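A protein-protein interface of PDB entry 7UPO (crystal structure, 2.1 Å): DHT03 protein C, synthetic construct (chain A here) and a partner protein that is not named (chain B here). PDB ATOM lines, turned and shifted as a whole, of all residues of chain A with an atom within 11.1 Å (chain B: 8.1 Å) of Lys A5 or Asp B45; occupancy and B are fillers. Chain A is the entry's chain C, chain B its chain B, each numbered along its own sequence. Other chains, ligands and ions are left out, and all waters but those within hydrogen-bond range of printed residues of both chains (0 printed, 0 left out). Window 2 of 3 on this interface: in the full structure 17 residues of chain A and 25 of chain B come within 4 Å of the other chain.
Among the printed residues, pairs that only touch across the chains: Gln A4 with Ser B46, Tyr A11 with Phe B49, Ile A8 with Ile B52, Tyr A11 with Ile B52, Lys A5 with Asp B45 and Ile A8 with Phe B49.
Printed residues of chain B within 4 Å of Gln A4: His B42, Asp B45 and Ser B46.
Lys A5 touches just one residue of chain B: Asp B45 (3.8 Å).
Glu A6 touches none of the printed residues of chain B.
Of the printed residues of chain B, Ile A8 touches Phe B49 (3.98 Å) and Ile B52 (3.6 Å).
Of the printed residues of chain B, Tyr A11 touches Phe B49 and Ile B52.
His B42 touches just one residue of chain A: Gln A4.
Gly B44 touches none of the printed residues of chain A.
Of chain A, only Gln A4 and Lys A5 come within 4 Å of Asp B45.
Ser B46 touches just one residue of chain A: Gln A4 (3.4 Å).
No residue of chain A comes within 4 Å of Ile B48.
Printed residues of chain A within 4 Å of Phe B49: Ile A8 and Tyr A11.
The nearest residue of chain B that does not touch Lys A5 is Leu B40 (6.1 Å).
The nearest residue of chain A that does not touch Asp B45 is Ile A8 (4.1 Å).
The nearest printed residue of chain A that does not touch Ile B52 is Leu A12 (4.3 Å).
N of Lys A5 lies close to OG of Ser A2, 3.5 Å away.
Printed residues of chain A that touch a printed residue of chain B: Gln A4, Lys A5, Ile A8 and Tyr A11.
Hydrophobic or aromatic side chains of chain A within 4 Å of the printed part of chain B: Ile A8 and Tyr A11.
Hydrophobic or aromatic side chains of chain B within 4 Å of the printed part of chain A: His B42, Phe B49 and Ile B52.
Among the printed residues, 8 pairs touch across the chains.
Among the printed residues, no Asp or Glu carboxylate lies within 4 Å of a Lys or Arg side-chain nitrogen of the other chain.
The side-chain amide oxygen of Gln A4 lies within hydrogen-bond range of a ring nitrogen (NE2) of His B42, at 3.2 Å.
The side-chain amide nitrogen (NE2) of Gln A4 is in hydrogen-bond range of the backbone carbonyl oxygen (O) of Asp B45 (3.4 Å).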
ATOM      1  N   SER A   2       1.172  19.625  -2.590  1.00  0.00           N
ATOM      2  CA  SER A   2       1.591  18.279  -2.214  1.00  0.00           C
ATOM      3  C   SER A   2       0.908  17.236  -3.101  1.00  0.00           C
ATOM      4  O   SER A   2      -0.114  17.519  -3.727  1.00  0.00           O
ATOM      5  CB  SER A   2       1.281  18.017  -0.737  1.00  0.00           C
ATOM      6  OG  SER A   2      -0.117  18.008  -0.502  1.00  0.00           O
ATOM      7  N   LYS A   3       1.480  16.029  -3.156  1.00  0.00           N
ATOM      8  CA  LYS A   3       0.924  14.987  -4.015  1.00  0.00           C
ATOM      9  C   LYS A   3      -0.385  14.435  -3.466  1.00  0.00           C
ATOM     10  O   LYS A   3      -1.197  13.900  -4.229  1.00  0.00           O
ATOM     11  CB  LYS A   3       1.941  13.864  -4.196  1.00  0.00           C
ATOM     12  CG  LYS A   3       3.240  14.317  -4.833  1.00  0.00           C
ATOM     13  CD  LYS A   3       4.386  13.395  -4.443  1.00  0.00           C
ATOM     14  CE  LYS A   3       5.725  13.913  -4.956  1.00  0.00           C
ATOM     15  NZ  LYS A   3       6.889  13.188  -4.361  1.00  0.00           N
ATOM     16  N   GLN A   4      -0.602  14.535  -2.152  1.00  0.00           N
ATOM     17  CA  GLN A   4      -1.889  14.125  -1.600  1.00  0.00           C
ATOM     18  C   GLN A   4      -2.996  15.080  -2.024  1.00  0.00           C
ATOM     19  O   GLN A   4      -4.132  14.648  -2.253  1.00  0.00           O
ATOM     20  CB  GLN A   4      -1.815  14.030  -0.075  1.00  0.00           C
ATOM     21  CG  GLN A   4      -3.109  13.553   0.574  1.00  0.00           C
ATOM     22  CD  GLN A   4      -2.880  12.826   1.886  1.00  0.00           C
ATOM     23  OE1 GLN A   4      -1.741  12.586   2.289  1.00  0.00           O
ATOM     24  NE2 GLN A   4      -3.966  12.464   2.556  1.00  0.00           N
ATOM     25  N   LYS A   5      -2.687  16.374  -2.137  1.00  0.00           N
ATOM     26  CA  LYS A   5      -3.645  17.302  -2.724  1.00  0.00           C
ATOM     27  C   LYS A   5      -3.870  17.002  -4.200  1.00  0.00           C
ATOM     28  O   LYS A   5      -4.956  17.267  -4.730  1.00  0.00           O
ATOM     29  CB  LYS A   5      -3.167  18.743  -2.544  1.00  0.00           C
ATOM     30  CG  LYS A   5      -3.113  19.217  -1.101  1.00  0.00           C
ATOM     31  CD  LYS A   5      -2.673  20.672  -1.021  1.00  0.00           C
ATOM     32  CE  LYS A   5      -2.712  21.190   0.406  1.00  0.00           C
ATOM     33  NZ  LYS A   5      -2.315  22.624   0.494  1.00  0.00           N
ATOM     34  N   GLU A   6      -2.860  16.445  -4.875  1.00  0.00           N
ATOM     35  CA  GLU A   6      -3.013  16.112  -6.287  1.00  0.00           C
ATOM     36  C   GLU A   6      -3.961  14.932  -6.472  1.00  0.00           C
ATOM     37  O   GLU A   6      -4.764  14.916  -7.411  1.00  0.00           O
ATOM     38  CB  GLU A   6      -1.646  15.816  -6.905  1.00  0.00           C
ATOM     39  CG  GLU A   6      -1.574  16.039  -8.410  1.00  0.00           C
ATOM     40  CD  GLU A   6      -1.454  17.506  -8.792  1.00  0.00           C
ATOM     41  OE1 GLU A   6      -1.465  18.368  -7.887  1.00  0.00           O
ATOM     42  OE2 GLU A   6      -1.344  17.798 -10.001  1.00  0.00           O
ATOM     43  N   ALA A   7      -3.883  13.936  -5.585  1.00  0.00           N
ATOM     44  CA  ALA A   7      -4.837  12.835  -5.627  1.00  0.00           C
ATOM     45  C   ALA A   7      -6.236  13.281  -5.224  1.00  0.00           C
ATOM     46  O   ALA A   7      -7.216  12.625  -5.594  1.00  0.00           O
ATOM     47  CB  ALA A   7      -4.372  11.694  -4.722  1.00  0.00           C
ATOM     48  N   ILE A   8      -6.348  14.374  -4.467  1.00  0.00           N
ATOM     49  CA  ILE A   8      -7.659  14.925  -4.147  1.00  0.00           C
ATOM     50  C   ILE A   8      -8.292  15.546  -5.386  1.00  0.00           C
ATOM     51  O   ILE A   8      -9.494  15.387  -5.631  1.00  0.00           O
ATOM     52  CB  ILE A   8      -7.543  15.939  -2.995  1.00  0.00           C
ATOM     53  CG1 ILE A   8      -7.303  15.214  -1.669  1.00  0.00           C
ATOM     54  CG2 ILE A   8      -8.785  16.818  -2.922  1.00  0.00           C
ATOM     55  CD1 ILE A   8      -7.101  16.145  -0.497  1.00  0.00           C
ATOM     56  N   LYS A   9      -7.496  16.253  -6.191  1.00  0.00           N
ATOM     57  CA  LYS A   9      -8.031  16.879  -7.396  1.00  0.00           C
ATOM     58  C   LYS A   9      -8.501  15.835  -8.397  1.00  0.00           C
ATOM     59  O   LYS A   9      -9.500  16.040  -9.096  1.00  0.00           O
ATOM     60  CB  LYS A   9      -6.984  17.793  -8.031  1.00  0.00           C
ATOM     61  CG  LYS A   9      -7.497  18.559  -9.240  1.00  0.00           C
ATOM     62  CD  LYS A   9      -6.454  19.520  -9.788  1.00  0.00           C
ATOM     63  CE  LYS A   9      -7.024  20.345 -10.936  1.00  0.00           C
ATOM     64  NZ  LYS A   9      -6.056  21.364 -11.433  1.00  0.00           N
ATOM     65  N   VAL A  10      -7.795  14.703  -8.476  1.00  0.00           N
ATOM     66  CA  VAL A  10      -8.191  13.637  -9.394  1.00  0.00           C
ATOM     67  C   VAL A  10      -9.551  13.073  -9.003  1.00  0.00           C
ATOM     68  O   VAL A  10     -10.429  12.877  -9.850  1.00  0.00           O
ATOM     69  CB  VAL A  10      -7.116  12.535  -9.428  1.00  0.00           C
ATOM     70  CG1 VAL A  10      -7.613  11.330 -10.207  1.00  0.00           C
ATOM     71  CG2 VAL A  10      -5.829  13.075 -10.027  1.00  0.00           C
ATOM     72  N   TYR A  11      -9.742  12.794  -7.709  1.00  0.00           N
ATOM     73  CA  TYR A  11     -11.002  12.211  -7.258  1.00  0.00           C
ATOM     74  C   TYR A  11     -12.167  13.169  -7.472  1.00  0.00           C
ATOM     75  O   TYR A  11     -13.273  12.742  -7.819  1.00  0.00           O
ATOM     76  CB  TYR A  11     -10.904  11.807  -5.786  1.00  0.00           C
ATOM     77  CG  TYR A  11     -10.479  10.371  -5.566  1.00  0.00           C
ATOM     78  CD1 TYR A  11     -10.195   9.538  -6.641  1.00  0.00           C
ATOM     79  CD2 TYR A  11     -10.380   9.843  -4.286  1.00  0.00           C
ATOM     80  CE1 TYR A  11      -9.812   8.224  -6.445  1.00  0.00           C
ATOM     81  CE2 TYR A  11      -9.998   8.528  -4.080  1.00  0.00           C
ATOM     82  CZ  TYR A  11      -9.715   7.724  -5.164  1.00  0.00           C
ATOM     83  OH  TYR A  11      -9.334   6.415  -4.962  1.00  0.00           O
ATOM     84  N   LEU A  12     -11.941  14.469  -7.262  1.00  0.00           N
ATOM     85  CA  LEU A  12     -12.986  15.449  -7.545  1.00  0.00           C
ATOM     86  C   LEU A  12     -13.325  15.473  -9.029  1.00  0.00           C
ATOM     87  O   LEU A  12     -14.491  15.652  -9.405  1.00  0.00           O
ATOM     88  CB  LEU A  12     -12.556  16.836  -7.071  1.00  0.00           C
ATOM     89  CG  LEU A  12     -12.494  17.060  -5.559  1.00  0.00           C
ATOM     90  CD1 LEU A  12     -12.051  18.481  -5.253  1.00  0.00           C
ATOM     91  CD2 LEU A  12     -13.842  16.762  -4.912  1.00  0.00           C
ATOM     92  N   GLU A  13     -12.320  15.295  -9.891  1.00  0.00           N
ATOM     93  CA  GLU A  13     -12.589  15.175 -11.321  1.00  0.00           C
ATOM     94  C   GLU A  13     -13.406  13.925 -11.621  1.00  0.00           C
ATOM     95  O   GLU A  13     -14.283  13.944 -12.492  1.00  0.00           O
ATOM     96  CB  GLU A  13     -11.277  15.155 -12.108  1.00  0.00           C
ATOM     97  CG  GLU A  13     -10.506  16.465 -12.088  1.00  0.00           C
ATOM     98  CD  GLU A  13      -9.250  16.416 -12.940  1.00  0.00           C
ATOM     99  OE1 GLU A  13      -9.209  15.620 -13.902  1.00  0.00           O
ATOM    100  OE2 GLU A  13      -8.299  17.172 -12.645  1.00  0.00           O
ATOM    101  N   LYS A  67      -2.571  12.037 -17.095  1.00  0.00           N
ATOM    102  CA  LYS A  67      -2.038  13.055 -16.197  1.00  0.00           C
ATOM    103  C   LYS A  67      -1.543  12.437 -14.895  1.00  0.00           C
ATOM    104  O   LYS A  67      -0.548  12.898 -14.325  1.00  0.00           O
ATOM    105  CB  LYS A  67      -3.099  14.121 -15.924  1.00  0.00           C
ATOM    106  CG  LYS A  67      -2.576  15.364 -15.214  1.00  0.00           C
ATOM    107  CD  LYS A  67      -2.872  15.335 -13.722  1.00  0.00           C
ATOM    108  CE  LYS A  67      -4.368  15.386 -13.454  1.00  0.00           C
ATOM    109  NZ  LYS A  67      -4.663  15.464 -12.000  1.00  0.00           N
ATOM    110  N   VAL A  68      -2.223  11.396 -14.410  1.00  0.00           N
ATOM    111  CA  VAL A  68      -1.773  10.725 -13.194  1.00  0.00           C
ATOM    112  C   VAL A  68      -0.503   9.928 -13.468  1.00  0.00           C
ATOM    113  O   VAL A  68       0.410   9.879 -12.636  1.00  0.00           O
ATOM    114  CB  VAL A  68      -2.894   9.836 -12.626  1.00  0.00           C
ATOM    115  CG1 VAL A  68      -2.389   9.052 -11.423  1.00  0.00           C
ATOM    116  CG2 VAL A  68      -4.095  10.683 -12.237  1.00  0.00           C
ATOM    117  N   ILE A  71       2.438  12.183 -13.284  1.00  0.00           N
ATOM    118  CA  ILE A  71       2.885  12.432 -11.918  1.00  0.00           C
ATOM    119  C   ILE A  71       3.649  11.227 -11.382  1.00  0.00           C
ATOM    120  O   ILE A  71       4.730  11.369 -10.800  1.00  0.00           O
ATOM    121  CB  ILE A  71       1.688  12.784 -11.018  1.00  0.00           C
ATOM    122  CG1 ILE A  71       0.866  13.909 -11.645  1.00  0.00           C
ATOM    123  CG2 ILE A  71       2.168  13.192  -9.638  1.00  0.00           C
ATOM    124  CD1 ILE A  71      -0.557  13.961 -11.152  1.00  0.00           C
ATOM    125  N   VAL A  75       7.359  11.044 -10.004  1.00  0.00           N
ATOM    126  CA  VAL A  75       7.597  10.653  -8.617  1.00  0.00           C
ATOM    127  C   VAL A  75       8.635   9.539  -8.548  1.00  0.00           C
ATOM    128  O   VAL A  75       9.603   9.615  -7.781  1.00  0.00           O
ATOM    129  CB  VAL A  75       6.279  10.237  -7.939  1.00  0.00           C
ATOM    130  CG1 VAL A  75       6.559   9.526  -6.623  1.00  0.00           C
ATOM    131  CG2 VAL A  75       5.397  11.452  -7.702  1.00  0.00           C
ATOM    132  N   ALA B  35     -12.328  23.304   3.139  1.00  0.00           N
ATOM    133  CA  ALA B  35     -11.051  22.786   3.614  1.00  0.00           C
ATOM    134  C   ALA B  35      -9.891  23.298   2.773  1.00  0.00           C
ATOM    135  O   ALA B  35      -8.777  23.456   3.285  1.00  0.00           O
ATOM    136  CB  ALA B  35     -11.072  21.258   3.618  1.00  0.00           C
ATOM    137  N   SER B  36     -10.130  23.561   1.487  1.00  0.00           N
ATOM    138  CA  SER B  36      -9.072  24.085   0.629  1.00  0.00           C
ATOM    139  C   SER B  36      -8.685  25.502   1.034  1.00  0.00           C
ATOM    140  O   SER B  36      -7.500  25.855   1.017  1.00  0.00           O
ATOM    141  CB  SER B  36      -9.518  24.048  -0.833  1.00  0.00           C
ATOM    142  OG  SER B  36      -8.559  24.661  -1.675  1.00  0.00           O
ATOM    143  N   ALA B  38      -8.667  26.740   3.919  1.00  0.00           N
ATOM    144  CA  ALA B  38      -8.146  26.763   5.278  1.00  0.00           C
ATOM    145  C   ALA B  38      -6.817  26.024   5.332  1.00  0.00           C
ATOM    146  O   ALA B  38      -6.621  25.026   4.630  1.00  0.00           O
ATOM    147  CB  ALA B  38      -9.137  26.134   6.262  1.00  0.00           C
ATOM    148  N   GLY B  39      -5.906  26.520   6.167  1.00  0.00           N
ATOM    149  CA  GLY B  39      -4.617  25.881   6.347  1.00  0.00           C
ATOM    150  C   GLY B  39      -4.726  24.566   7.089  1.00  0.00           C
ATOM    151  O   GLY B  39      -4.891  24.547   8.313  1.00  0.00           O
ATOM    152  N   LEU B  40      -4.634  23.458   6.361  1.00  0.00           N
ATOM    153  CA  LEU B  40      -4.854  22.135   6.924  1.00  0.00           C
ATOM    154  C   LEU B  40      -3.538  21.420   7.198  1.00  0.00           C
ATOM    155  O   LEU B  40      -2.555  21.575   6.469  1.00  0.00           O
ATOM    156  CB  LEU B  40      -5.711  21.283   5.987  1.00  0.00           C
ATOM    157  CG  LEU B  40      -7.221  21.305   6.220  1.00  0.00           C
ATOM    158  CD1 LEU B  40      -7.918  20.384   5.235  1.00  0.00           C
ATOM    159  CD2 LEU B  40      -7.542  20.904   7.652  1.00  0.00           C
ATOM    160  N   ASP B  41      -3.539  20.627   8.266  1.00  0.00           N
ATOM    161  CA  ASP B  41      -2.418  19.761   8.584  1.00  0.00           C
ATOM    162  C   ASP B  41      -2.373  18.589   7.602  1.00  0.00           C
ATOM    163  O   ASP B  41      -3.284  18.383   6.794  1.00  0.00           O
ATOM    164  CB  ASP B  41      -2.538  19.259  10.023  1.00  0.00           C
ATOM    165  CG  ASP B  41      -1.237  18.703  10.565  1.00  0.00           C
ATOM    166  OD1 ASP B  41      -0.251  18.634   9.800  1.00  0.00           O
ATOM    167  OD2 ASP B  41      -1.200  18.337  11.758  1.00  0.00           O
ATOM    168  N   HIS B  42      -1.287  17.814   7.668  1.00  0.00           N
ATOM    169  CA  HIS B  42      -1.213  16.610   6.850  1.00  0.00           C
ATOM    170  C   HIS B  42      -2.255  15.585   7.281  1.00  0.00           C
ATOM    171  O   HIS B  42      -2.717  14.786   6.457  1.00  0.00           O
ATOM    172  CB  HIS B  42       0.190  16.004   6.913  1.00  0.00           C
ATOM    173  CG  HIS B  42       0.362  14.800   6.041  1.00  0.00           C
ATOM    174  ND1 HIS B  42       0.778  13.580   6.529  1.00  0.00           N
ATOM    175  CD2 HIS B  42       0.159  14.624   4.714  1.00  0.00           C
ATOM    176  CE1 HIS B  42       0.833  12.708   5.539  1.00  0.00           C
ATOM    177  NE2 HIS B  42       0.461  13.315   4.426  1.00  0.00           N
ATOM    178  N   GLU B  43      -2.636  15.594   8.562  1.00  0.00           N
ATOM    179  CA  GLU B  43      -3.742  14.765   9.023  1.00  0.00           C
ATOM    180  C   GLU B  43      -5.086  15.330   8.582  1.00  0.00           C
ATOM    181  O   GLU B  43      -6.036  14.568   8.370  1.00  0.00           O
ATOM    182  CB  GLU B  43      -3.703  14.634  10.546  1.00  0.00           C
ATOM    183  CG  GLU B  43      -2.348  14.243  11.105  1.00  0.00           C
ATOM    184  CD  GLU B  43      -2.319  14.253  12.621  1.00  0.00           C
ATOM    185  OE1 GLU B  43      -3.376  14.006  13.239  1.00  0.00           O
ATOM    186  OE2 GLU B  43      -1.240  14.517  13.195  1.00  0.00           O
ATOM    187  N   GLY B  44      -5.186  16.655   8.454  1.00  0.00           N
ATOM    188  CA  GLY B  44      -6.407  17.248   7.936  1.00  0.00           C
ATOM    189  C   GLY B  44      -6.628  16.919   6.472  1.00  0.00           C
ATOM    190  O   GLY B  44      -7.757  16.660   6.049  1.00  0.00           O
ATOM    191  N   ASP B  45      -5.552  16.924   5.681  1.00  0.00           N
ATOM    192  CA  ASP B  45      -5.652  16.463   4.301  1.00  0.00           C
ATOM    193  C   ASP B  45      -5.987  14.980   4.236  1.00  0.00           C
ATOM    194  O   ASP B  45      -6.588  14.521   3.259  1.00  0.00           O
ATOM    195  CB  ASP B  45      -4.346  16.741   3.556  1.00  0.00           C
ATOM    196  CG  ASP B  45      -4.016  18.219   3.490  1.00  0.00           C
ATOM    197  OD1 ASP B  45      -4.902  19.041   3.803  1.00  0.00           O
ATOM    198  OD2 ASP B  45      -2.869  18.557   3.127  1.00  0.00           O
ATOM    199  N   SER B  46      -5.610  14.218   5.266  1.00  0.00           N
ATOM    200  CA  SER B  46      -5.896  12.788   5.282  1.00  0.00           C
ATOM    201  C   SER B  46      -7.387  12.526   5.453  1.00  0.00           C
ATOM    202  O   SER B  46      -7.980  11.744   4.700  1.00  0.00           O
ATOM    203  CB  SER B  46      -5.100  12.107   6.395  1.00  0.00           C
ATOM    204  OG  SER B  46      -5.539  10.775   6.595  1.00  0.00           O
ATOM    205  N   ARG B  47      -8.014  13.169   6.442  1.00  0.00           N
ATOM    206  CA  ARG B  47      -9.442  12.958   6.659  1.00  0.00           C
ATOM    207  C   ARG B  47     -10.266  13.482   5.490  1.00  0.00           C
ATOM    208  O   ARG B  47     -11.323  12.920   5.180  1.00  0.00           O
ATOM    209  CB  ARG B  47      -9.888  13.615   7.968  1.00  0.00           C
ATOM    210  CG  ARG B  47      -9.892  15.136   7.950  1.00  0.00           C
ATOM    211  CD  ARG B  47     -10.385  15.712   9.269  1.00  0.00           C
ATOM    212  NE  ARG B  47     -11.713  15.217   9.626  1.00  0.00           N
ATOM    213  CZ  ARG B  47     -12.408  15.636  10.678  1.00  0.00           C
ATOM    214  NH1 ARG B  47     -11.907  16.566  11.481  1.00  0.00           N
ATOM    215  NH2 ARG B  47     -13.609  15.128  10.927  1.00  0.00           N
ATOM    216  N   ILE B  48      -9.797  14.539   4.824  1.00  0.00           N
ATOM    217  CA  ILE B  48     -10.509  15.057   3.662  1.00  0.00           C
ATOM    218  C   ILE B  48     -10.468  14.047   2.524  1.00  0.00           C
ATOM    219  O   ILE B  48     -11.489  13.767   1.886  1.00  0.00           O
ATOM    220  CB  ILE B  48      -9.927  16.417   3.234  1.00  0.00           C
ATOM    221  CG1 ILE B  48     -10.318  17.499   4.241  1.00  0.00           C
ATOM    222  CG2 ILE B  48     -10.400  16.787   1.837  1.00  0.00           C
ATOM    223  CD1 ILE B  48     -11.815  17.681   4.385  1.00  0.00           C
ATOM    224  N   PHE B  49      -9.291  13.472   2.262  1.00  0.00           N
ATOM    225  CA  PHE B  49      -9.185  12.476   1.200  1.00  0.00           C
ATOM    226  C   PHE B  49     -10.014  11.238   1.518  1.00  0.00           C
ATOM    227  O   PHE B  49     -10.665  10.676   0.631  1.00  0.00           O
ATOM    228  CB  PHE B  49      -7.726  12.087   0.966  1.00  0.00           C
ATOM    229  CG  PHE B  49      -7.558  10.983  -0.040  1.00  0.00           C
ATOM    230  CD1 PHE B  49      -7.627  11.253  -1.397  1.00  0.00           C
ATOM    231  CD2 PHE B  49      -7.350   9.676   0.370  1.00  0.00           C
ATOM    232  CE1 PHE B  49      -7.484  10.241  -2.328  1.00  0.00           C
ATOM    233  CE2 PHE B  49      -7.206   8.659  -0.557  1.00  0.00           C
ATOM    234  CZ  PHE B  49      -7.273   8.943  -1.908  1.00  0.00           C
ATOM    235  N   LYS B  50      -9.993  10.789   2.776  1.00  0.00           N
ATOM    236  CA  LYS B  50     -10.795   9.630   3.158  1.00  0.00           C
ATOM    237  C   LYS B  50     -12.282   9.914   2.988  1.00  0.00           C
ATOM    238  O   LYS B  50     -13.053   9.027   2.603  1.00  0.00           O
ATOM    239  CB  LYS B  50     -10.477   9.225   4.598  1.00  0.00           C
ATOM    240  CG  LYS B  50      -9.118   8.552   4.759  1.00  0.00           C
ATOM    241  CD  LYS B  50      -8.853   8.128   6.199  1.00  0.00           C
ATOM    242  CE  LYS B  50      -8.545   9.323   7.087  1.00  0.00           C
ATOM    243  NZ  LYS B  50      -8.122   8.909   8.453  1.00  0.00           N
ATOM    244  N   LYS B  51     -12.700  11.150   3.264  1.00  0.00           N
ATOM    245  CA  LYS B  51     -14.086  11.538   3.029  1.00  0.00           C
ATOM    246  C   LYS B  51     -14.416  11.489   1.541  1.00  0.00           C
ATOM    247  O   LYS B  51     -15.464  10.969   1.141  1.00  0.00           O
ATOM    248  CB  LYS B  51     -14.334  12.937   3.591  1.00  0.00           C
ATOM    249  CG  LYS B  51     -15.796  13.321   3.749  1.00  0.00           C
ATOM    250  CD  LYS B  51     -16.439  12.586   4.915  1.00  0.00           C
ATOM    251  CE  LYS B  51     -17.670  13.321   5.421  1.00  0.00           C
ATOM    252  NZ  LYS B  51     -17.326  14.639   6.033  1.00  0.00           N
ATOM    253  N   ILE B  52     -13.523  12.027   0.706  1.00  0.00           N
ATOM    254  CA  ILE B  52     -13.732  11.998  -0.738  1.00  0.00           C
ATOM    255  C   ILE B  52     -13.700  10.566  -1.254  1.00  0.00           C
ATOM    256  O   ILE B  52     -14.466  10.197  -2.154  1.00  0.00           O
ATOM    257  CB  ILE B  52     -12.683  12.877  -1.445  1.00  0.00           C
ATOM    258  CG1 ILE B  52     -12.756  14.314  -0.934  1.00  0.00           C
ATOM    259  CG2 ILE B  52     -12.890  12.858  -2.947  1.00  0.00           C
ATOM    260  CD1 ILE B  52     -11.701  15.213  -1.520  1.00  0.00           C
